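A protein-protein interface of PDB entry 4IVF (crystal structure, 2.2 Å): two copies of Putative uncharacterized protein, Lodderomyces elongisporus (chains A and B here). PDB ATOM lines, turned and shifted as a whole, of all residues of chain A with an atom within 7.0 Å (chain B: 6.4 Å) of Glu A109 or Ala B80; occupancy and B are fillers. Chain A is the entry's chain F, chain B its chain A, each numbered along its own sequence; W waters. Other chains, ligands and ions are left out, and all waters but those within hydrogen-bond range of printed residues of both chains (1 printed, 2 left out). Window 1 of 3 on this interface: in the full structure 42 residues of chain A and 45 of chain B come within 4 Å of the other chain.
Of chain B, only Leu B75, Ser B76, Gln B77 and Ala B80 come within 4 Å of Glu A109. Of chain A, only Glu A109 (3.7 Å) comes within 4 Å of Ala B80. Of the printed residues of chain B, Phe A113 touches Gln B77. Of the printed residues of chain A, Gln B83 touches Leu A108 (3.7 Å). Printed residues of chain B within 4 Å of Leu A108: Gln B83. Of the printed residues of chain A, Tyr B84 touches Tyr A105. Of the printed residues of chain A, Gln B77 touches Glu A109 (3.4 Å), Ile A112 (3.5 Å) and Phe A113 (3.5 Å). Ala A177 touches none of the printed residues of chain B. The nearest residue of chain B that does not touch Glu A109 is Val B74 (4.1 Å). The nearest printed residue of chain A that does not touch Gln B77 is Leu A108 (5.6 Å).
Position printed for both chains: 111. Of the 12 pairs that touch across the chains among the printed residues, none has its exchanged pair printed and touching as well.
Water W1 lies within hydrogen-bond range of the side-chain hydroxyl of Ser B76, the backbone carbonyl oxygen of Leu B52 and the side-chain carboxylate of Glu A109.
The side-chain amide nitrogen (ND2) of Asn B53 lies close to the side-chain hydroxyl (OG) of Ser B76, at 3.3 Å. OE1 of Glu A109 is in salt-bridge range of NZ of Lys A106 (2.8 Å).
O of Val B74 is in hydrogen-bond range of NZ of Lys A106 (3.2 Å). The side-chain carboxylate (OE1) of Glu A109 lies within hydrogen-bond range of the backbone NH (N) of Ser B76, at 3.1 Å.
Leu B75 touches Tyr A105. CE1 of Tyr A105 touches CA of Tyr B84, 3.6 Å away. CD2 of Leu A108 touches CG of Gln B83, 3.7 Å away. Glu A109 touches Leu B75. Glu A109 touches Gln B77. Ala B80 touches Glu A109 (CB to CA, 3.7 Å). Ile A112 touches Gln B77 (CG2 to OE1, 3.5 Å). Ile A112 touches Gly B79 (CG2 to CA, 3.9 Å). Phe A113 touches Gln B77. Pro B54 touches Ile A157.
Of the 17 printed residues of chain B, 9 touch a printed residue of chain A. Of the 14 printed residues of chain A, 7 touch a printed residue of chain B. Hydrophobic or aromatic side chains of chain A that line the printed part of chain B: Tyr A105, Leu A108, Ile A112, Phe A113 and Ile A157. Along chain A the printed residues that touch a printed residue of chain B span positions 105 to 157. Among the printed residues, 12 pairs touch across the chains. Among the printed residues, no Asp or Glu carboxylate lies within 4 Å of a Lys or Arg side-chain nitrogen of the other chain.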
ATOM      1  N   GLU A 103      -5.503 -14.239  28.862  1.00  0.00           N
ATOM      2  CA  GLU A 103      -4.462 -15.158  28.428  1.00  0.00           C
ATOM      3  C   GLU A 103      -4.377 -15.255  26.895  1.00  0.00           C
ATOM      4  O   GLU A 103      -3.301 -15.401  26.348  1.00  0.00           O
ATOM      5  CB  GLU A 103      -4.644 -16.546  29.055  1.00  0.00           C
ATOM      6  CG  GLU A 103      -4.497 -16.596  30.596  1.00  0.00           C
ATOM      7  CD  GLU A 103      -5.785 -16.206  31.367  1.00  0.00           C
ATOM      8  OE1 GLU A 103      -6.833 -15.871  30.746  1.00  0.00           O
ATOM      9  OE2 GLU A 103      -5.734 -16.242  32.620  1.00  0.00           O
ATOM     10  N   TYR A 104      -5.516 -15.188  26.214  1.00  0.00           N
ATOM     11  CA  TYR A 104      -5.537 -15.173  24.756  1.00  0.00           C
ATOM     12  C   TYR A 104      -4.729 -13.996  24.218  1.00  0.00           C
ATOM     13  O   TYR A 104      -3.875 -14.153  23.336  1.00  0.00           O
ATOM     14  CB  TYR A 104      -6.978 -15.106  24.243  1.00  0.00           C
ATOM     15  CG  TYR A 104      -7.086 -14.828  22.769  1.00  0.00           C
ATOM     16  CD1 TYR A 104      -7.027 -15.862  21.848  1.00  0.00           C
ATOM     17  CD2 TYR A 104      -7.245 -13.524  22.292  1.00  0.00           C
ATOM     18  CE1 TYR A 104      -7.116 -15.615  20.486  1.00  0.00           C
ATOM     19  CE2 TYR A 104      -7.339 -13.264  20.927  1.00  0.00           C
ATOM     20  CZ  TYR A 104      -7.274 -14.316  20.029  1.00  0.00           C
ATOM     21  OH  TYR A 104      -7.371 -14.087  18.672  1.00  0.00           O
ATOM     22  N   TYR A 105      -4.990 -12.817  24.775  1.00  0.00           N
ATOM     23  CA  TYR A 105      -4.256 -11.617  24.395  1.00  0.00           C
ATOM     24  C   TYR A 105      -2.769 -11.579  24.797  1.00  0.00           C
ATOM     25  O   TYR A 105      -1.938 -11.089  24.032  1.00  0.00           O
ATOM     26  CB  TYR A 105      -5.027 -10.360  24.821  1.00  0.00           C
ATOM     27  CG  TYR A 105      -6.277 -10.214  23.994  1.00  0.00           C
ATOM     28  CD1 TYR A 105      -6.204  -9.864  22.644  1.00  0.00           C
ATOM     29  CD2 TYR A 105      -7.529 -10.489  24.533  1.00  0.00           C
ATOM     30  CE1 TYR A 105      -7.359  -9.750  21.865  1.00  0.00           C
ATOM     31  CE2 TYR A 105      -8.687 -10.380  23.767  1.00  0.00           C
ATOM     32  CZ  TYR A 105      -8.595 -10.014  22.437  1.00  0.00           C
ATOM     33  OH  TYR A 105      -9.745  -9.921  21.688  1.00  0.00           O
ATOM     34  N   LYS A 106      -2.422 -12.089  25.974  1.00  0.00           N
ATOM     35  CA  LYS A 106      -1.006 -12.166  26.323  1.00  0.00           C
ATOM     36  C   LYS A 106      -0.264 -13.101  25.351  1.00  0.00           C
ATOM     37  O   LYS A 106       0.875 -12.843  25.019  1.00  0.00           O
ATOM     38  CB  LYS A 106      -0.771 -12.629  27.771  1.00  0.00           C
ATOM     39  CG  LYS A 106      -1.332 -11.705  28.867  1.00  0.00           C
ATOM     40  CD  LYS A 106      -0.931 -10.237  28.720  1.00  0.00           C
ATOM     41  CE  LYS A 106       0.557  -9.996  28.892  1.00  0.00           C
ATOM     42  NZ  LYS A 106       0.873  -8.525  29.000  1.00  0.00           N
ATOM     43  N   THR A 107      -0.916 -14.184  24.929  1.00  0.00           N
ATOM     44  CA  THR A 107      -0.350 -15.102  23.947  1.00  0.00           C
ATOM     45  C   THR A 107      -0.050 -14.337  22.670  1.00  0.00           C
ATOM     46  O   THR A 107       1.025 -14.469  22.074  1.00  0.00           O
ATOM     47  CB  THR A 107      -1.326 -16.258  23.619  1.00  0.00           C
ATOM     48  OG1 THR A 107      -1.428 -17.126  24.752  1.00  0.00           O
ATOM     49  CG2 THR A 107      -0.831 -17.074  22.424  1.00  0.00           C
ATOM     50  N   LEU A 108      -1.009 -13.510  22.286  1.00  0.00           N
ATOM     51  CA  LEU A 108      -0.898 -12.683  21.098  1.00  0.00           C
ATOM     52  C   LEU A 108       0.242 -11.667  21.247  1.00  0.00           C
ATOM     53  O   LEU A 108       1.041 -11.474  20.326  1.00  0.00           O
ATOM     54  CB  LEU A 108      -2.229 -11.980  20.824  1.00  0.00           C
ATOM     55  CG  LEU A 108      -2.489 -11.579  19.376  1.00  0.00           C
ATOM     56  CD1 LEU A 108      -2.517 -12.821  18.490  1.00  0.00           C
ATOM     57  CD2 LEU A 108      -3.797 -10.793  19.265  1.00  0.00           C
ATOM     58  N   GLU A 109       0.325 -11.026  22.409  1.00  0.00           N
ATOM     59  CA  GLU A 109       1.411 -10.086  22.654  1.00  0.00           C
ATOM     60  C   GLU A 109       2.800 -10.731  22.533  1.00  0.00           C
ATOM     61  O   GLU A 109       3.724 -10.133  22.001  1.00  0.00           O
ATOM     62  CB  GLU A 109       1.258  -9.427  24.025  1.00  0.00           C
ATOM     63  CG  GLU A 109       2.496  -8.661  24.472  1.00  0.00           C
ATOM     64  CD  GLU A 109       2.328  -8.040  25.843  1.00  0.00           C
ATOM     65  OE1 GLU A 109       1.169  -7.907  26.291  1.00  0.00           O
ATOM     66  OE2 GLU A 109       3.351  -7.678  26.465  1.00  0.00           O
ATOM     67  N   TYR A 110       2.958 -11.950  23.030  1.00  0.00           N
ATOM     68  CA  TYR A 110       4.277 -12.567  23.011  1.00  0.00           C
ATOM     69  C   TYR A 110       4.582 -13.201  21.642  1.00  0.00           C
ATOM     70  O   TYR A 110       5.733 -13.205  21.184  1.00  0.00           O
ATOM     71  CB  TYR A 110       4.421 -13.562  24.167  1.00  0.00           C
ATOM     72  CG  TYR A 110       4.314 -12.911  25.534  1.00  0.00           C
ATOM     73  CD1 TYR A 110       4.705 -11.585  25.734  1.00  0.00           C
ATOM     74  CD2 TYR A 110       3.826 -13.623  26.630  1.00  0.00           C
ATOM     75  CE1 TYR A 110       4.602 -10.992  26.998  1.00  0.00           C
ATOM     76  CE2 TYR A 110       3.718 -13.042  27.884  1.00  0.00           C
ATOM     77  CZ  TYR A 110       4.106 -11.732  28.062  1.00  0.00           C
ATOM     78  OH  TYR A 110       3.989 -11.166  29.307  1.00  0.00           O
ATOM     79  N   LEU A 111       3.550 -13.723  20.990  1.00  0.00           N
ATOM     80  CA  LEU A 111       3.677 -14.144  19.602  1.00  0.00           C
ATOM     81  C   LEU A 111       4.152 -12.980  18.728  1.00  0.00           C
ATOM     82  O   LEU A 111       5.114 -13.119  17.979  1.00  0.00           O
ATOM     83  CB  LEU A 111       2.358 -14.697  19.055  1.00  0.00           C
ATOM     84  CG  LEU A 111       2.382 -14.962  17.532  1.00  0.00           C
ATOM     85  CD1 LEU A 111       3.369 -16.060  17.166  1.00  0.00           C
ATOM     86  CD2 LEU A 111       0.995 -15.310  16.998  1.00  0.00           C
ATOM     87  N   ILE A 112       3.477 -11.838  18.816  1.00  0.00           N
ATOM     88  CA  ILE A 112       3.849 -10.684  17.993  1.00  0.00           C
ATOM     89  C   ILE A 112       5.267 -10.209  18.324  1.00  0.00           C
ATOM     90  O   ILE A 112       6.059  -9.922  17.419  1.00  0.00           O
ATOM     91  CB  ILE A 112       2.815  -9.522  18.086  1.00  0.00           C
ATOM     92  CG1 ILE A 112       1.448  -9.959  17.542  1.00  0.00           C
ATOM     93  CG2 ILE A 112       3.314  -8.277  17.357  1.00  0.00           C
ATOM     94  CD1 ILE A 112       1.511 -10.709  16.253  1.00  0.00           C
ATOM     95  N   PHE A 113       5.594 -10.177  19.617  1.00  0.00           N
ATOM     96  CA  PHE A 113       6.943  -9.861  20.087  1.00  0.00           C
ATOM     97  C   PHE A 113       7.988 -10.760  19.415  1.00  0.00           C
ATOM     98  O   PHE A 113       9.032 -10.288  18.973  1.00  0.00           O
ATOM     99  CB  PHE A 113       7.020 -10.009  21.614  1.00  0.00           C
ATOM    100  CG  PHE A 113       8.386  -9.721  22.207  1.00  0.00           C
ATOM    101  CD1 PHE A 113       9.176  -8.692  21.724  1.00  0.00           C
ATOM    102  CD2 PHE A 113       8.852 -10.463  23.285  1.00  0.00           C
ATOM    103  CE1 PHE A 113      10.420  -8.432  22.287  1.00  0.00           C
ATOM    104  CE2 PHE A 113      10.089 -10.200  23.855  1.00  0.00           C
ATOM    105  CZ  PHE A 113      10.874  -9.180  23.350  1.00  0.00           C
ATOM    106  N   GLN A 114       7.703 -12.053  19.340  1.00  0.00           N
ATOM    107  CA  GLN A 114       8.593 -12.971  18.648  1.00  0.00           C
ATOM    108  C   GLN A 114       8.735 -12.605  17.162  1.00  0.00           C
ATOM    109  O   GLN A 114       9.846 -12.432  16.687  1.00  0.00           O
ATOM    110  CB  GLN A 114       8.131 -14.427  18.814  1.00  0.00           C
ATOM    111  CG  GLN A 114       9.181 -15.462  18.383  1.00  0.00           C
ATOM    112  CD  GLN A 114       9.371 -15.514  16.865  1.00  0.00           C
ATOM    113  OE1 GLN A 114       8.402 -15.624  16.109  1.00  0.00           O
ATOM    114  NE2 GLN A 114      10.620 -15.403  16.418  1.00  0.00           N
ATOM    115  N   ILE A 157       9.969 -12.852  31.075  1.00  0.00           N
ATOM    116  CA  ILE A 157       8.592 -13.294  30.863  1.00  0.00           C
ATOM    117  C   ILE A 157       8.341 -14.638  31.553  1.00  0.00           C
ATOM    118  O   ILE A 157       7.366 -14.794  32.313  1.00  0.00           O
ATOM    119  CB  ILE A 157       8.246 -13.357  29.348  1.00  0.00           C
ATOM    120  CG1 ILE A 157       8.233 -11.950  28.769  1.00  0.00           C
ATOM    121  CG2 ILE A 157       6.891 -13.995  29.123  1.00  0.00           C
ATOM    122  CD1 ILE A 157       8.050 -11.900  27.296  1.00  0.00           C
ATOM    123  N   ALA A 177       2.929 -18.823  20.940  1.00  0.00           N
ATOM    124  CA  ALA A 177       4.032 -17.942  21.286  1.00  0.00           C
ATOM    125  C   ALA A 177       5.287 -18.761  21.597  1.00  0.00           C
ATOM    126  O   ALA A 177       6.376 -18.432  21.141  1.00  0.00           O
ATOM    127  CB  ALA A 177       3.659 -17.029  22.448  1.00  0.00           C
ATOM    128  N   LEU B  52       5.274  -3.392  33.803  1.00  0.00           N
ATOM    129  CA  LEU B  52       4.091  -3.413  32.944  1.00  0.00           C
ATOM    130  C   LEU B  52       4.399  -4.116  31.602  1.00  0.00           C
ATOM    131  O   LEU B  52       3.592  -4.906  31.088  1.00  0.00           O
ATOM    132  CB  LEU B  52       3.583  -1.990  32.673  1.00  0.00           C
ATOM    133  CG  LEU B  52       3.150  -1.128  33.860  1.00  0.00           C
ATOM    134  CD1 LEU B  52       2.814   0.287  33.406  1.00  0.00           C
ATOM    135  CD2 LEU B  52       1.986  -1.767  34.596  1.00  0.00           C
ATOM    136  N   ASN B  53       5.578  -3.826  31.056  1.00  0.00           N
ATOM    137  CA  ASN B  53       6.005  -4.363  29.765  1.00  0.00           C
ATOM    138  C   ASN B  53       7.459  -4.796  29.831  1.00  0.00           C
ATOM    139  O   ASN B  53       8.347  -3.951  29.746  1.00  0.00           O
ATOM    140  CB  ASN B  53       5.832  -3.299  28.668  1.00  0.00           C
ATOM    141  CG  ASN B  53       6.356  -3.752  27.302  1.00  0.00           C
ATOM    142  OD1 ASN B  53       6.591  -4.931  27.067  1.00  0.00           O
ATOM    143  ND2 ASN B  53       6.531  -2.803  26.401  1.00  0.00           N
ATOM    144  N   PRO B  54       7.701  -6.118  29.943  1.00  0.00           N
ATOM    145  CA  PRO B  54       9.041  -6.729  30.062  1.00  0.00           C
ATOM    146  C   PRO B  54      10.004  -6.251  28.966  1.00  0.00           C
ATOM    147  O   PRO B  54      11.206  -6.108  29.212  1.00  0.00           O
ATOM    148  CB  PRO B  54       8.778  -8.228  29.862  1.00  0.00           C
ATOM    149  CG  PRO B  54       7.299  -8.415  30.001  1.00  0.00           C
ATOM    150  CD  PRO B  54       6.640  -7.114  29.692  1.00  0.00           C
ATOM    151  N   VAL B  74      -3.287  -5.038  30.825  1.00  0.00           N
ATOM    152  CA  VAL B  74      -2.097  -4.358  30.331  1.00  0.00           C
ATOM    153  C   VAL B  74      -1.607  -5.093  29.083  1.00  0.00           C
ATOM    154  O   VAL B  74      -1.420  -6.305  29.104  1.00  0.00           O
ATOM    155  CB  VAL B  74      -0.983  -4.367  31.384  1.00  0.00           C
ATOM    156  CG1 VAL B  74       0.292  -3.704  30.831  1.00  0.00           C
ATOM    157  CG2 VAL B  74      -1.467  -3.695  32.655  1.00  0.00           C
ATOM    158  N   LEU B  75      -1.401  -4.368  27.996  1.00  0.00           N
ATOM    159  CA  LEU B  75      -1.082  -5.016  26.730  1.00  0.00           C
ATOM    160  C   LEU B  75      -0.041  -4.236  25.944  1.00  0.00           C
ATOM    161  O   LEU B  75      -0.158  -3.019  25.791  1.00  0.00           O
ATOM    162  CB  LEU B  75      -2.354  -5.139  25.895  1.00  0.00           C
ATOM    163  CG  LEU B  75      -2.336  -6.236  24.851  1.00  0.00           C
ATOM    164  CD1 LEU B  75      -2.129  -7.560  25.566  1.00  0.00           C
ATOM    165  CD2 LEU B  75      -3.646  -6.220  24.071  1.00  0.00           C
ATOM    166  N   SER B  76       0.971  -4.933  25.443  1.00  0.00           N
ATOM    167  CA  SER B  76       2.000  -4.289  24.615  1.00  0.00           C
ATOM    168  C   SER B  76       2.067  -4.934  23.223  1.00  0.00           C
ATOM    169  O   SER B  76       1.321  -5.879  22.961  1.00  0.00           O
ATOM    170  CB  SER B  76       3.368  -4.336  25.309  1.00  0.00           C
ATOM    171  OG  SER B  76       3.368  -3.555  26.500  1.00  0.00           O
ATOM    172  N   GLN B  77       2.971  -4.435  22.370  1.00  0.00           N
ATOM    173  CA  GLN B  77       3.095  -4.830  20.945  1.00  0.00           C
ATOM    174  C   GLN B  77       1.968  -4.268  20.085  1.00  0.00           C
ATOM    175  O   GLN B  77       0.811  -4.710  20.187  1.00  0.00           O
ATOM    176  CB  GLN B  77       3.203  -6.355  20.750  1.00  0.00           C
ATOM    177  CG  GLN B  77       4.539  -6.923  21.189  1.00  0.00           C
ATOM    178  CD  GLN B  77       5.672  -6.382  20.338  1.00  0.00           C
ATOM    179  OE1 GLN B  77       5.493  -6.122  19.148  1.00  0.00           O
ATOM    180  NE2 GLN B  77       6.827  -6.182  20.943  1.00  0.00           N
ATOM    181  N   THR B  78       2.294  -3.285  19.250  1.00  0.00           N
ATOM    182  CA  THR B  78       1.275  -2.674  18.385  1.00  0.00           C
ATOM    183  C   THR B  78       0.426  -3.726  17.658  1.00  0.00           C
ATOM    184  O   THR B  78      -0.772  -3.555  17.504  1.00  0.00           O
ATOM    185  CB  THR B  78       1.863  -1.718  17.339  1.00  0.00           C
ATOM    186  OG1 THR B  78       2.792  -2.429  16.519  1.00  0.00           O
ATOM    187  CG2 THR B  78       2.541  -0.531  17.993  1.00  0.00           C
ATOM    188  N   GLY B  79       1.041  -4.819  17.233  1.00  0.00           N
ATOM    189  CA  GLY B  79       0.281  -5.878  16.595  1.00  0.00           C
ATOM    190  C   GLY B  79      -0.847  -6.400  17.470  1.00  0.00           C
ATOM    191  O   GLY B  79      -1.968  -6.595  16.993  1.00  0.00           O
ATOM    192  N   ALA B  80      -0.553  -6.630  18.753  1.00  0.00           N
ATOM    193  CA  ALA B  80      -1.533  -7.199  19.671  1.00  0.00           C
ATOM    194  C   ALA B  80      -2.566  -6.159  20.112  1.00  0.00           C
ATOM    195  O   ALA B  80      -3.757  -6.443  20.175  1.00  0.00           O
ATOM    196  CB  ALA B  80      -0.841  -7.812  20.879  1.00  0.00           C
ATOM    197  N   ILE B  81      -2.106  -4.952  20.400  1.00  0.00           N
ATOM    198  CA  ILE B  81      -3.006  -3.895  20.855  1.00  0.00           C
ATOM    199  C   ILE B  81      -4.050  -3.578  19.791  1.00  0.00           C
ATOM    200  O   ILE B  81      -5.233  -3.462  20.099  1.00  0.00           O
ATOM    201  CB  ILE B  81      -2.223  -2.625  21.196  1.00  0.00           C
ATOM    202  CG1 ILE B  81      -1.268  -2.903  22.353  1.00  0.00           C
ATOM    203  CG2 ILE B  81      -3.159  -1.468  21.491  1.00  0.00           C
ATOM    204  CD1 ILE B  81      -0.158  -1.884  22.450  1.00  0.00           C
ATOM    205  N   LEU B  82      -3.608  -3.453  18.540  1.00  0.00           N
ATOM    206  CA  LEU B  82      -4.512  -3.154  17.442  1.00  0.00           C
ATOM    207  C   LEU B  82      -5.576  -4.234  17.309  1.00  0.00           C
ATOM    208  O   LEU B  82      -6.772  -3.933  17.182  1.00  0.00           O
ATOM    209  CB  LEU B  82      -3.747  -2.992  16.122  1.00  0.00           C
ATOM    210  CG  LEU B  82      -2.994  -1.669  15.947  1.00  0.00           C
ATOM    211  CD1 LEU B  82      -2.196  -1.661  14.645  1.00  0.00           C
ATOM    212  CD2 LEU B  82      -3.950  -0.472  16.027  1.00  0.00           C
ATOM    213  N   GLN B  83      -5.140  -5.487  17.349  1.00  0.00           N
ATOM    214  CA  GLN B  83      -6.067  -6.599  17.264  1.00  0.00           C
ATOM    215  C   GLN B  83      -7.066  -6.567  18.428  1.00  0.00           C
ATOM    216  O   GLN B  83      -8.283  -6.690  18.219  1.00  0.00           O
ATOM    217  CB  GLN B  83      -5.310  -7.926  17.222  1.00  0.00           C
ATOM    218  CG  GLN B  83      -6.190  -9.133  16.954  1.00  0.00           C
ATOM    219  CD  GLN B  83      -6.941  -9.052  15.624  1.00  0.00           C
ATOM    220  OE1 GLN B  83      -6.450  -8.492  14.642  1.00  0.00           O
ATOM    221  NE2 GLN B  83      -8.136  -9.624  15.594  1.00  0.00           N
ATOM    222  N   TYR B  84      -6.543  -6.388  19.642  1.00  0.00           N
ATOM    223  CA  TYR B  84      -7.383  -6.260  20.826  1.00  0.00           C
ATOM    224  C   TYR B  84      -8.426  -5.151  20.691  1.00  0.00           C
ATOM    225  O   TYR B  84      -9.581  -5.358  20.994  1.00  0.00           O
ATOM    226  CB  TYR B  84      -6.549  -6.034  22.103  1.00  0.00           C
ATOM    227  CG  TYR B  84      -7.408  -5.603  23.290  1.00  0.00           C
ATOM    228  CD1 TYR B  84      -8.126  -6.539  24.027  1.00  0.00           C
ATOM    229  CD2 TYR B  84      -7.523  -4.263  23.642  1.00  0.00           C
ATOM    230  CE1 TYR B  84      -8.928  -6.151  25.104  1.00  0.00           C
ATOM    231  CE2 TYR B  84      -8.327  -3.860  24.704  1.00  0.00           C
ATOM    232  CZ  TYR B  84      -9.021  -4.810  25.435  1.00  0.00           C
ATOM    233  OH  TYR B  84      -9.816  -4.421  26.485  1.00  0.00           O
ATOM    234  N   LEU B  85      -8.010  -3.972  20.249  1.00  0.00           N
ATOM    235  CA  LEU B  85      -8.945  -2.858  20.073  1.00  0.00           C
ATOM    236  C   LEU B  85     -10.044  -3.172  19.047  1.00  0.00           C
ATOM    237  O   LEU B  85     -11.228  -2.880  19.277  1.00  0.00           O
ATOM    238  CB  LEU B  85      -8.189  -1.577  19.706  1.00  0.00           C
ATOM    239  CG  LEU B  85      -7.195  -1.111  20.782  1.00  0.00           C
ATOM    240  CD1 LEU B  85      -6.448   0.165  20.357  1.00  0.00           C
ATOM    241  CD2 LEU B  85      -7.912  -0.922  22.135  1.00  0.00           C
ATOM    242  N   LEU B 111      -1.233  -7.169   8.597  1.00  0.00           N
ATOM    243  CA  LEU B 111      -0.873  -6.505   9.853  1.00  0.00           C
ATOM    244  C   LEU B 111       0.453  -7.075  10.335  1.00  0.00           C
ATOM    245  O   LEU B 111       1.389  -6.340  10.654  1.00  0.00           O
ATOM    246  CB  LEU B 111      -1.941  -6.702  10.943  1.00  0.00           C
ATOM    247  CG  LEU B 111      -1.509  -6.319  12.375  1.00  0.00           C
ATOM    248  CD1 LEU B 111      -1.144  -4.860  12.505  1.00  0.00           C
ATOM    249  CD2 LEU B 111      -2.588  -6.653  13.365  1.00  0.00           C
ATOM    250  N   VAL B 115       4.176  -5.437  11.064  1.00  0.00           N
ATOM    251  CA  VAL B 115       4.930  -5.414  12.328  1.00  0.00           C
ATOM    252  C   VAL B 115       6.192  -6.261  12.270  1.00  0.00           C
ATOM    253  O   VAL B 115       7.174  -5.951  12.928  1.00  0.00           O
ATOM    254  CB  VAL B 115       4.094  -5.854  13.568  1.00  0.00           C
ATOM    255  CG1 VAL B 115       2.982  -4.854  13.873  1.00  0.00           C
ATOM    256  CG2 VAL B 115       3.547  -7.243  13.386  1.00  0.00           C
HETATM  257  O   HOH W   1       2.697  -5.534  28.391  1.00  0.00           O
